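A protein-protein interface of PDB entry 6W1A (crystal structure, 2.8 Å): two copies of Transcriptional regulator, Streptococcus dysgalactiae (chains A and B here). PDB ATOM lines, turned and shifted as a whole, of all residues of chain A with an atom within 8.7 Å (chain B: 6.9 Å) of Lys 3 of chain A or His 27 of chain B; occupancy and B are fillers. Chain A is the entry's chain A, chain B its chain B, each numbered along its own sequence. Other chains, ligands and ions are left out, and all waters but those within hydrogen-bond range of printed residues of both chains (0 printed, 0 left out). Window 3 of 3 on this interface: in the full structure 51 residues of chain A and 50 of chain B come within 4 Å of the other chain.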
ATOM      1  N   LYS A   3     -18.638 -17.757  20.554  1.00  0.00           N
ATOM      2  CA  LYS A   3     -18.314 -16.926  19.402  1.00  0.00           C
ATOM      3  C   LYS A   3     -19.259 -15.732  19.311  1.00  0.00           C
ATOM      4  O   LYS A   3     -19.877 -15.498  18.269  1.00  0.00           O
ATOM      5  CB  LYS A   3     -18.375 -17.748  18.113  1.00  0.00           C
ATOM      6  CG  LYS A   3     -17.536 -17.190  16.973  1.00  0.00           C
ATOM      7  CD  LYS A   3     -17.328 -18.233  15.889  1.00  0.00           C
ATOM      8  CE  LYS A   3     -16.636 -19.467  16.444  1.00  0.00           C
ATOM      9  NZ  LYS A   3     -16.483 -20.531  15.417  1.00  0.00           N
ATOM     10  N   GLU A   4     -19.375 -14.997  20.422  1.00  0.00           N
ATOM     11  CA  GLU A   4     -20.136 -13.747  20.483  1.00  0.00           C
ATOM     12  C   GLU A   4     -21.640 -13.992  20.304  1.00  0.00           C
ATOM     13  O   GLU A   4     -22.319 -13.299  19.545  1.00  0.00           O
ATOM     14  CB  GLU A   4     -19.608 -12.735  19.457  1.00  0.00           C
ATOM     15  CG  GLU A   4     -20.037 -11.289  19.675  1.00  0.00           C
ATOM     16  CD  GLU A   4     -20.081 -10.501  18.378  1.00  0.00           C
ATOM     17  OE1 GLU A   4     -21.140 -10.497  17.715  1.00  0.00           O
ATOM     18  OE2 GLU A   4     -19.057  -9.877  18.025  1.00  0.00           O
ATOM     19  N   LEU A   5     -22.163 -14.991  21.018  1.00  0.00           N
ATOM     20  CA  LEU A   5     -23.603 -15.214  21.042  1.00  0.00           C
ATOM     21  C   LEU A   5     -24.291 -14.484  22.186  1.00  0.00           C
ATOM     22  O   LEU A   5     -25.515 -14.318  22.145  1.00  0.00           O
ATOM     23  CB  LEU A   5     -23.921 -16.708  21.170  1.00  0.00           C
ATOM     24  CG  LEU A   5     -23.463 -17.692  20.100  1.00  0.00           C
ATOM     25  CD1 LEU A   5     -23.170 -19.048  20.717  1.00  0.00           C
ATOM     26  CD2 LEU A   5     -24.533 -17.807  19.043  1.00  0.00           C
ATOM     27  N   GLY A   6     -23.540 -14.051  23.198  1.00  0.00           N
ATOM     28  CA  GLY A   6     -24.130 -13.268  24.270  1.00  0.00           C
ATOM     29  C   GLY A   6     -24.498 -11.862  23.842  1.00  0.00           C
ATOM     30  O   GLY A   6     -25.501 -11.306  24.301  1.00  0.00           O
ATOM     31  N   LYS A   7     -23.679 -11.265  22.973  1.00  0.00           N
ATOM     32  CA  LYS A   7     -23.937  -9.927  22.453  1.00  0.00           C
ATOM     33  C   LYS A   7     -25.350  -9.803  21.897  1.00  0.00           C
ATOM     34  O   LYS A   7     -26.117  -8.926  22.309  1.00  0.00           O
ATOM     35  CB  LYS A   7     -22.901  -9.587  21.382  1.00  0.00           C
ATOM     36  CG  LYS A   7     -22.925  -8.143  20.894  1.00  0.00           C
ATOM     37  CD  LYS A   7     -22.238  -8.031  19.535  1.00  0.00           C
ATOM     38  CE  LYS A   7     -21.992  -6.584  19.136  1.00  0.00           C
ATOM     39  NZ  LYS A   7     -21.426  -6.470  17.761  1.00  0.00           N
ATOM     40  N   THR A   8     -25.702 -10.654  20.931  1.00  0.00           N
ATOM     41  CA  THR A   8     -27.019 -10.528  20.316  1.00  0.00           C
ATOM     42  C   THR A   8     -28.127 -10.955  21.271  1.00  0.00           C
ATOM     43  O   THR A   8     -29.236 -10.410  21.213  1.00  0.00           O
ATOM     44  CB  THR A   8     -27.079 -11.327  19.013  1.00  0.00           C
ATOM     45  OG1 THR A   8     -26.836 -12.713  19.280  1.00  0.00           O
ATOM     46  CG2 THR A   8     -26.023 -10.806  18.053  1.00  0.00           C
ATOM     47  N   PHE A  36     -21.908 -14.126  29.961  1.00  0.00           N
ATOM     48  CA  PHE A  36     -22.163 -14.654  28.624  1.00  0.00           C
ATOM     49  C   PHE A  36     -22.522 -13.527  27.670  1.00  0.00           C
ATOM     50  O   PHE A  36     -22.068 -13.501  26.522  1.00  0.00           O
ATOM     51  CB  PHE A  36     -23.280 -15.698  28.655  1.00  0.00           C
ATOM     52  CG  PHE A  36     -23.749 -16.130  27.292  1.00  0.00           C
ATOM     53  CD1 PHE A  36     -25.046 -15.877  26.877  1.00  0.00           C
ATOM     54  CD2 PHE A  36     -22.892 -16.796  26.426  1.00  0.00           C
ATOM     55  CE1 PHE A  36     -25.483 -16.275  25.625  1.00  0.00           C
ATOM     56  CE2 PHE A  36     -23.320 -17.196  25.173  1.00  0.00           C
ATOM     57  CZ  PHE A  36     -24.618 -16.937  24.772  1.00  0.00           C
ATOM     58  N   GLY A  39     -19.322 -11.622  26.274  1.00  0.00           N
ATOM     59  CA  GLY A  39     -18.256 -12.327  25.591  1.00  0.00           C
ATOM     60  C   GLY A  39     -17.155 -12.810  26.500  1.00  0.00           C
ATOM     61  O   GLY A  39     -16.054 -13.111  26.026  1.00  0.00           O
ATOM     62  N   SER A  41     -17.838 -15.379  28.926  1.00  0.00           N
ATOM     63  CA  SER A  41     -18.096 -16.792  29.151  1.00  0.00           C
ATOM     64  C   SER A  41     -19.090 -17.258  28.098  1.00  0.00           C
ATOM     65  O   SER A  41     -19.827 -16.454  27.521  1.00  0.00           O
ATOM     66  CB  SER A  41     -18.610 -17.047  30.577  1.00  0.00           C
ATOM     67  OG  SER A  41     -19.145 -18.351  30.723  1.00  0.00           O
ATOM     68  N   GLU A  42     -19.098 -18.562  27.836  1.00  0.00           N
ATOM     69  CA  GLU A  42     -20.008 -19.154  26.863  1.00  0.00           C
ATOM     70  C   GLU A  42     -20.843 -20.211  27.566  1.00  0.00           C
ATOM     71  O   GLU A  42     -20.302 -21.058  28.285  1.00  0.00           O
ATOM     72  CB  GLU A  42     -19.255 -19.760  25.674  1.00  0.00           C
ATOM     73  CG  GLU A  42     -18.626 -18.725  24.752  1.00  0.00           C
ATOM     74  CD  GLU A  42     -19.652 -17.940  23.950  1.00  0.00           C
ATOM     75  OE1 GLU A  42     -19.685 -16.698  24.095  1.00  0.00           O
ATOM     76  OE2 GLU A  42     -20.410 -18.559  23.167  1.00  0.00           O
ATOM     77  N   ILE A  43     -22.155 -20.162  27.358  1.00  0.00           N
ATOM     78  CA  ILE A  43     -23.077 -21.022  28.076  1.00  0.00           C
ATOM     79  C   ILE A  43     -23.392 -22.253  27.235  1.00  0.00           C
ATOM     80  O   ILE A  43     -23.259 -22.262  26.007  1.00  0.00           O
ATOM     81  CB  ILE A  43     -24.374 -20.270  28.460  1.00  0.00           C
ATOM     82  CG1 ILE A  43     -25.030 -19.663  27.215  1.00  0.00           C
ATOM     83  CG2 ILE A  43     -24.077 -19.197  29.496  1.00  0.00           C
ATOM     84  CD1 ILE A  43     -26.453 -19.208  27.434  1.00  0.00           C
ATOM     85  N   HIS A  66     -28.322 -12.907  15.124  1.00  0.00           N
ATOM     86  CA  HIS A  66     -26.884 -12.868  15.396  1.00  0.00           C
ATOM     87  C   HIS A  66     -26.115 -12.622  14.102  1.00  0.00           C
ATOM     88  O   HIS A  66     -25.559 -11.537  13.889  1.00  0.00           O
ATOM     89  CB  HIS A  66     -26.466 -14.195  16.060  1.00  0.00           C
ATOM     90  CG  HIS A  66     -24.988 -14.371  16.264  1.00  0.00           C
ATOM     91  ND1 HIS A  66     -24.091 -13.325  16.254  1.00  0.00           N
ATOM     92  CD2 HIS A  66     -24.254 -15.489  16.488  1.00  0.00           C
ATOM     93  CE1 HIS A  66     -22.871 -13.789  16.461  1.00  0.00           C
ATOM     94  NE2 HIS A  66     -22.943 -15.100  16.605  1.00  0.00           N
ATOM     95  N   SER A  67     -26.069 -13.643  13.253  1.00  0.00           N
ATOM     96  CA  SER A  67     -25.639 -13.585  11.864  1.00  0.00           C
ATOM     97  C   SER A  67     -26.790 -14.151  11.046  1.00  0.00           C
ATOM     98  O   SER A  67     -27.732 -14.716  11.601  1.00  0.00           O
ATOM     99  CB  SER A  67     -24.331 -14.350  11.630  1.00  0.00           C
ATOM    100  OG  SER A  67     -23.741 -13.992  10.389  1.00  0.00           O
ATOM    101  N   HIS A  70     -24.503 -17.379   8.552  1.00  0.00           N
ATOM    102  CA  HIS A  70     -23.762 -17.983   9.648  1.00  0.00           C
ATOM    103  C   HIS A  70     -23.286 -19.365   9.229  1.00  0.00           C
ATOM    104  O   HIS A  70     -22.102 -19.687   9.345  1.00  0.00           O
ATOM    105  CB  HIS A  70     -24.651 -18.065  10.894  1.00  0.00           C
ATOM    106  CG  HIS A  70     -23.892 -18.050  12.182  1.00  0.00           C
ATOM    107  ND1 HIS A  70     -22.916 -17.118  12.455  1.00  0.00           N
ATOM    108  CD2 HIS A  70     -23.946 -18.866  13.262  1.00  0.00           C
ATOM    109  CE1 HIS A  70     -22.407 -17.353  13.651  1.00  0.00           C
ATOM    110  NE2 HIS A  70     -23.013 -18.409  14.162  1.00  0.00           N
ATOM    111  N   ALA B  24     -13.887 -32.819  14.328  1.00  0.00           N
ATOM    112  CA  ALA B  24     -12.905 -32.214  15.219  1.00  0.00           C
ATOM    113  C   ALA B  24     -12.149 -31.090  14.518  1.00  0.00           C
ATOM    114  O   ALA B  24     -11.872 -31.149  13.317  1.00  0.00           O
ATOM    115  CB  ALA B  24     -11.925 -33.269  15.724  1.00  0.00           C
ATOM    116  N   ASP B  25     -11.810 -30.059  15.287  1.00  0.00           N
ATOM    117  CA  ASP B  25     -11.149 -28.874  14.749  1.00  0.00           C
ATOM    118  C   ASP B  25     -10.481 -28.121  15.897  1.00  0.00           C
ATOM    119  O   ASP B  25     -10.356 -28.636  17.013  1.00  0.00           O
ATOM    120  CB  ASP B  25     -12.149 -27.983  14.004  1.00  0.00           C
ATOM    121  CG  ASP B  25     -13.367 -27.635  14.845  1.00  0.00           C
ATOM    122  OD1 ASP B  25     -13.644 -28.346  15.836  1.00  0.00           O
ATOM    123  OD2 ASP B  25     -14.045 -26.641  14.517  1.00  0.00           O
ATOM    124  N   GLU B  26     -10.040 -26.891  15.610  1.00  0.00           N
ATOM    125  CA  GLU B  26      -9.448 -26.042  16.639  1.00  0.00           C
ATOM    126  C   GLU B  26     -10.425 -25.762  17.773  1.00  0.00           C
ATOM    127  O   GLU B  26     -10.003 -25.531  18.911  1.00  0.00           O
ATOM    128  CB  GLU B  26      -8.982 -24.720  16.025  1.00  0.00           C
ATOM    129  CG  GLU B  26      -8.470 -24.841  14.598  1.00  0.00           C
ATOM    130  CD  GLU B  26      -8.649 -23.559  13.798  1.00  0.00           C
ATOM    131  OE1 GLU B  26      -9.131 -22.561  14.371  1.00  0.00           O
ATOM    132  OE2 GLU B  26      -8.311 -23.554  12.594  1.00  0.00           O
ATOM    133  N   HIS B  27     -11.727 -25.786  17.488  1.00  0.00           N
ATOM    134  CA  HIS B  27     -12.717 -25.320  18.450  1.00  0.00           C
ATOM    135  C   HIS B  27     -13.156 -26.396  19.432  1.00  0.00           C
ATOM    136  O   HIS B  27     -13.580 -26.063  20.545  1.00  0.00           O
ATOM    137  CB  HIS B  27     -13.935 -24.761  17.712  1.00  0.00           C
ATOM    138  CG  HIS B  27     -13.616 -23.590  16.838  1.00  0.00           C
ATOM    139  ND1 HIS B  27     -13.375 -23.714  15.487  1.00  0.00           N
ATOM    140  CD2 HIS B  27     -13.475 -22.274  17.125  1.00  0.00           C
ATOM    141  CE1 HIS B  27     -13.113 -22.524  14.977  1.00  0.00           C
ATOM    142  NE2 HIS B  27     -13.166 -21.633  15.950  1.00  0.00           N
ATOM    143  N   LEU B  28     -13.068 -27.671  19.065  1.00  0.00           N
ATOM    144  CA  LEU B  28     -13.425 -28.721  20.008  1.00  0.00           C
ATOM    145  C   LEU B  28     -12.673 -29.995  19.656  1.00  0.00           C
ATOM    146  O   LEU B  28     -12.651 -30.420  18.498  1.00  0.00           O
ATOM    147  CB  LEU B  28     -14.939 -28.966  20.025  1.00  0.00           C
ATOM    148  CG  LEU B  28     -15.451 -30.062  20.963  1.00  0.00           C
ATOM    149  CD1 LEU B  28     -15.428 -29.582  22.403  1.00  0.00           C
ATOM    150  CD2 LEU B  28     -16.861 -30.472  20.575  1.00  0.00           C
ATOM    151  N   SER B  29     -12.072 -30.591  20.684  1.00  0.00           N
ATOM    152  CA  SER B  29     -11.482 -31.925  20.687  1.00  0.00           C
ATOM    153  C   SER B  29     -12.428 -33.004  20.184  1.00  0.00           C
ATOM    154  O   SER B  29     -13.649 -32.838  20.211  1.00  0.00           O
ATOM    155  CB  SER B  29     -11.004 -32.273  22.097  1.00  0.00           C
ATOM    156  OG  SER B  29     -11.963 -31.877  23.067  1.00  0.00           O
ATOM    157  N   ILE B  43     -21.447 -29.594  25.787  1.00  0.00           N
ATOM    158  CA  ILE B  43     -20.501 -28.687  25.147  1.00  0.00           C
ATOM    159  C   ILE B  43     -21.071 -27.271  25.116  1.00  0.00           C
ATOM    160  O   ILE B  43     -22.276 -27.044  25.269  1.00  0.00           O
ATOM    161  CB  ILE B  43     -20.106 -29.134  23.718  1.00  0.00           C
ATOM    162  CG1 ILE B  43     -19.913 -30.643  23.607  1.00  0.00           C
ATOM    163  CG2 ILE B  43     -18.818 -28.471  23.268  1.00  0.00           C
ATOM    164  CD1 ILE B  43     -20.225 -31.149  22.213  1.00  0.00           C
ATOM    165  N   SER B  44     -20.167 -26.309  24.939  1.00  0.00           N
ATOM    166  CA  SER B  44     -20.513 -24.943  24.572  1.00  0.00           C
ATOM    167  C   SER B  44     -21.507 -24.928  23.415  1.00  0.00           C
ATOM    168  O   SER B  44     -21.528 -25.827  22.569  1.00  0.00           O
ATOM    169  CB  SER B  44     -19.240 -24.184  24.188  1.00  0.00           C
ATOM    170  OG  SER B  44     -19.524 -23.031  23.420  1.00  0.00           O
ATOM    171  N   SER B  46     -21.743 -22.437  21.010  1.00  0.00           N
ATOM    172  CA  SER B  46     -21.014 -22.105  19.790  1.00  0.00           C
ATOM    173  C   SER B  46     -20.359 -23.339  19.172  1.00  0.00           C
ATOM    174  O   SER B  46     -20.296 -23.480  17.947  1.00  0.00           O
ATOM    175  CB  SER B  46     -19.980 -21.025  20.080  1.00  0.00           C
ATOM    176  OG  SER B  46     -18.976 -21.018  19.081  1.00  0.00           O
ATOM    177  N   ARG B  47     -19.840 -24.237  20.010  1.00  0.00           N
ATOM    178  CA  ARG B  47     -19.179 -25.434  19.502  1.00  0.00           C
ATOM    179  C   ARG B  47     -20.174 -26.470  19.004  1.00  0.00           C
ATOM    180  O   ARG B  47     -19.848 -27.240  18.096  1.00  0.00           O
ATOM    181  CB  ARG B  47     -18.270 -26.043  20.579  1.00  0.00           C
ATOM    182  CG  ARG B  47     -17.138 -25.122  20.983  1.00  0.00           C
ATOM    183  CD  ARG B  47     -16.365 -25.659  22.169  1.00  0.00           C
ATOM    184  NE  ARG B  47     -15.031 -25.067  22.239  1.00  0.00           N
ATOM    185  CZ  ARG B  47     -14.367 -24.855  23.370  1.00  0.00           C
ATOM    186  NH1 ARG B  47     -14.919 -25.179  24.530  1.00  0.00           N
ATOM    187  NH2 ARG B  47     -13.154 -24.317  23.342  1.00  0.00           N
ATOM    188  N   ASN B  50     -21.009 -25.248  15.650  1.00  0.00           N
ATOM    189  CA  ASN B  50     -19.926 -25.561  14.722  1.00  0.00           C
ATOM    190  C   ASN B  50     -19.986 -27.017  14.280  1.00  0.00           C
ATOM    191  O   ASN B  50     -19.797 -27.323  13.097  1.00  0.00           O
ATOM    192  CB  ASN B  50     -18.579 -25.247  15.368  1.00  0.00           C
ATOM    193  CG  ASN B  50     -17.469 -25.093  14.353  1.00  0.00           C
ATOM    194  OD1 ASN B  50     -16.709 -26.027  14.103  1.00  0.00           O
ATOM    195  ND2 ASN B  50     -17.373 -23.911  13.755  1.00  0.00           N
ATOM    196  N   LYS B  54     -20.552 -28.308  10.280  1.00  0.00           N
ATOM    197  CA  LYS B  54     -19.775 -29.258   9.497  1.00  0.00           C
ATOM    198  C   LYS B  54     -20.644 -30.403   8.993  1.00  0.00           C
ATOM    199  O   LYS B  54     -20.321 -31.025   7.975  1.00  0.00           O
ATOM    200  CB  LYS B  54     -18.622 -29.795  10.340  1.00  0.00           C
ATOM    201  CG  LYS B  54     -17.658 -28.732  10.837  1.00  0.00           C
ATOM    202  CD  LYS B  54     -16.420 -29.385  11.441  1.00  0.00           C
ATOM    203  CE  LYS B  54     -15.591 -28.399  12.250  1.00  0.00           C
ATOM    204  NZ  LYS B  54     -14.920 -27.387  11.385  1.00  0.00           N
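Position printed for both chains: 43. Of the 6 pairs that touch across the chains among the printed residues, none has its exchanged pair printed and touching as well.
NZ of Lys 3 of chain A touches NE2 of His 27 of chain B (3.5 Å). Lys 3 of chain A touches Ser 46 of chain B (CB to OG, 3.5 Å). Lys 3 of chain A touches Asn 50 of chain B (NZ to ND2, 3.9 Å). Leu 5 of chain A touches Ser 46 of chain B (CD1 to N, 3.7 Å). Ser 44 of chain B touches Glu 42 of chain A (OG to CB, 3.98 Å). Ser 46 of chain B touches Glu 42 of chain A.
Of the printed residues of chain B, Lys 3 of chain A touches His 27, Ser 46 and Asn 50. Of the printed residues of chain B, Glu 42 of chain A touches Ser 44 (3.98 Å) and Ser 46 (3.97 Å). Printed residues of chain B within 4 Å of Leu 5 of chain A: Ser 46. Printed residues of chain A within 4 Å of Asn 50 of chain B: Lys 3. Printed residues of chain A within 4 Å of Ser 46 of chain B: Lys 3 (3.5 Å), Leu 5 (3.7 Å) and Glu 42 (3.97 Å). Ile 43 of chain A touches none of the printed residues of chain B. Ile 43 of chain B touches none of the printed residues of chain A. The nearest printed residue of chain A that does not touch His 27 of chain B is Glu 42 of chain A (9.8 Å).
The backbone NH of Lys 3 of chain A sits at hydrogen-bond distance from the side-chain carboxylate of Glu 42 of chain A. OG of Ser 44 of chain B is in hydrogen-bond range of N of Ser 46 of chain B (3.3 Å). OD1 of Asn 50 of chain B sits close to OD2 of Asp 25 of chain B (2.8 Å). The side-chain carboxylate of Asp 25 of chain B lies within hydrogen-bond range of a ring nitrogen (ND1) of His 27 of chain B (3.2 Å). The guanidinium group of Arg 47 of chain B sits at hydrogen-bond distance from the backbone carbonyl oxygen of His 27 of chain B.
Of the 12 printed residues of chain B, 4 touch a printed residue of chain A. Hydrophobic or aromatic side chains of chain B within 4 Å of the printed part of chain A: His 27. Hydrophobic or aromatic side chains of chain A within 4 Å of the printed part of chain B: Leu 5. Among the printed residues, 6 pairs touch across the chains. Among the printed residues, no Asp or Glu carboxylate lies within 4 Å of a Lys or Arg side-chain nitrogen of the other chain.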
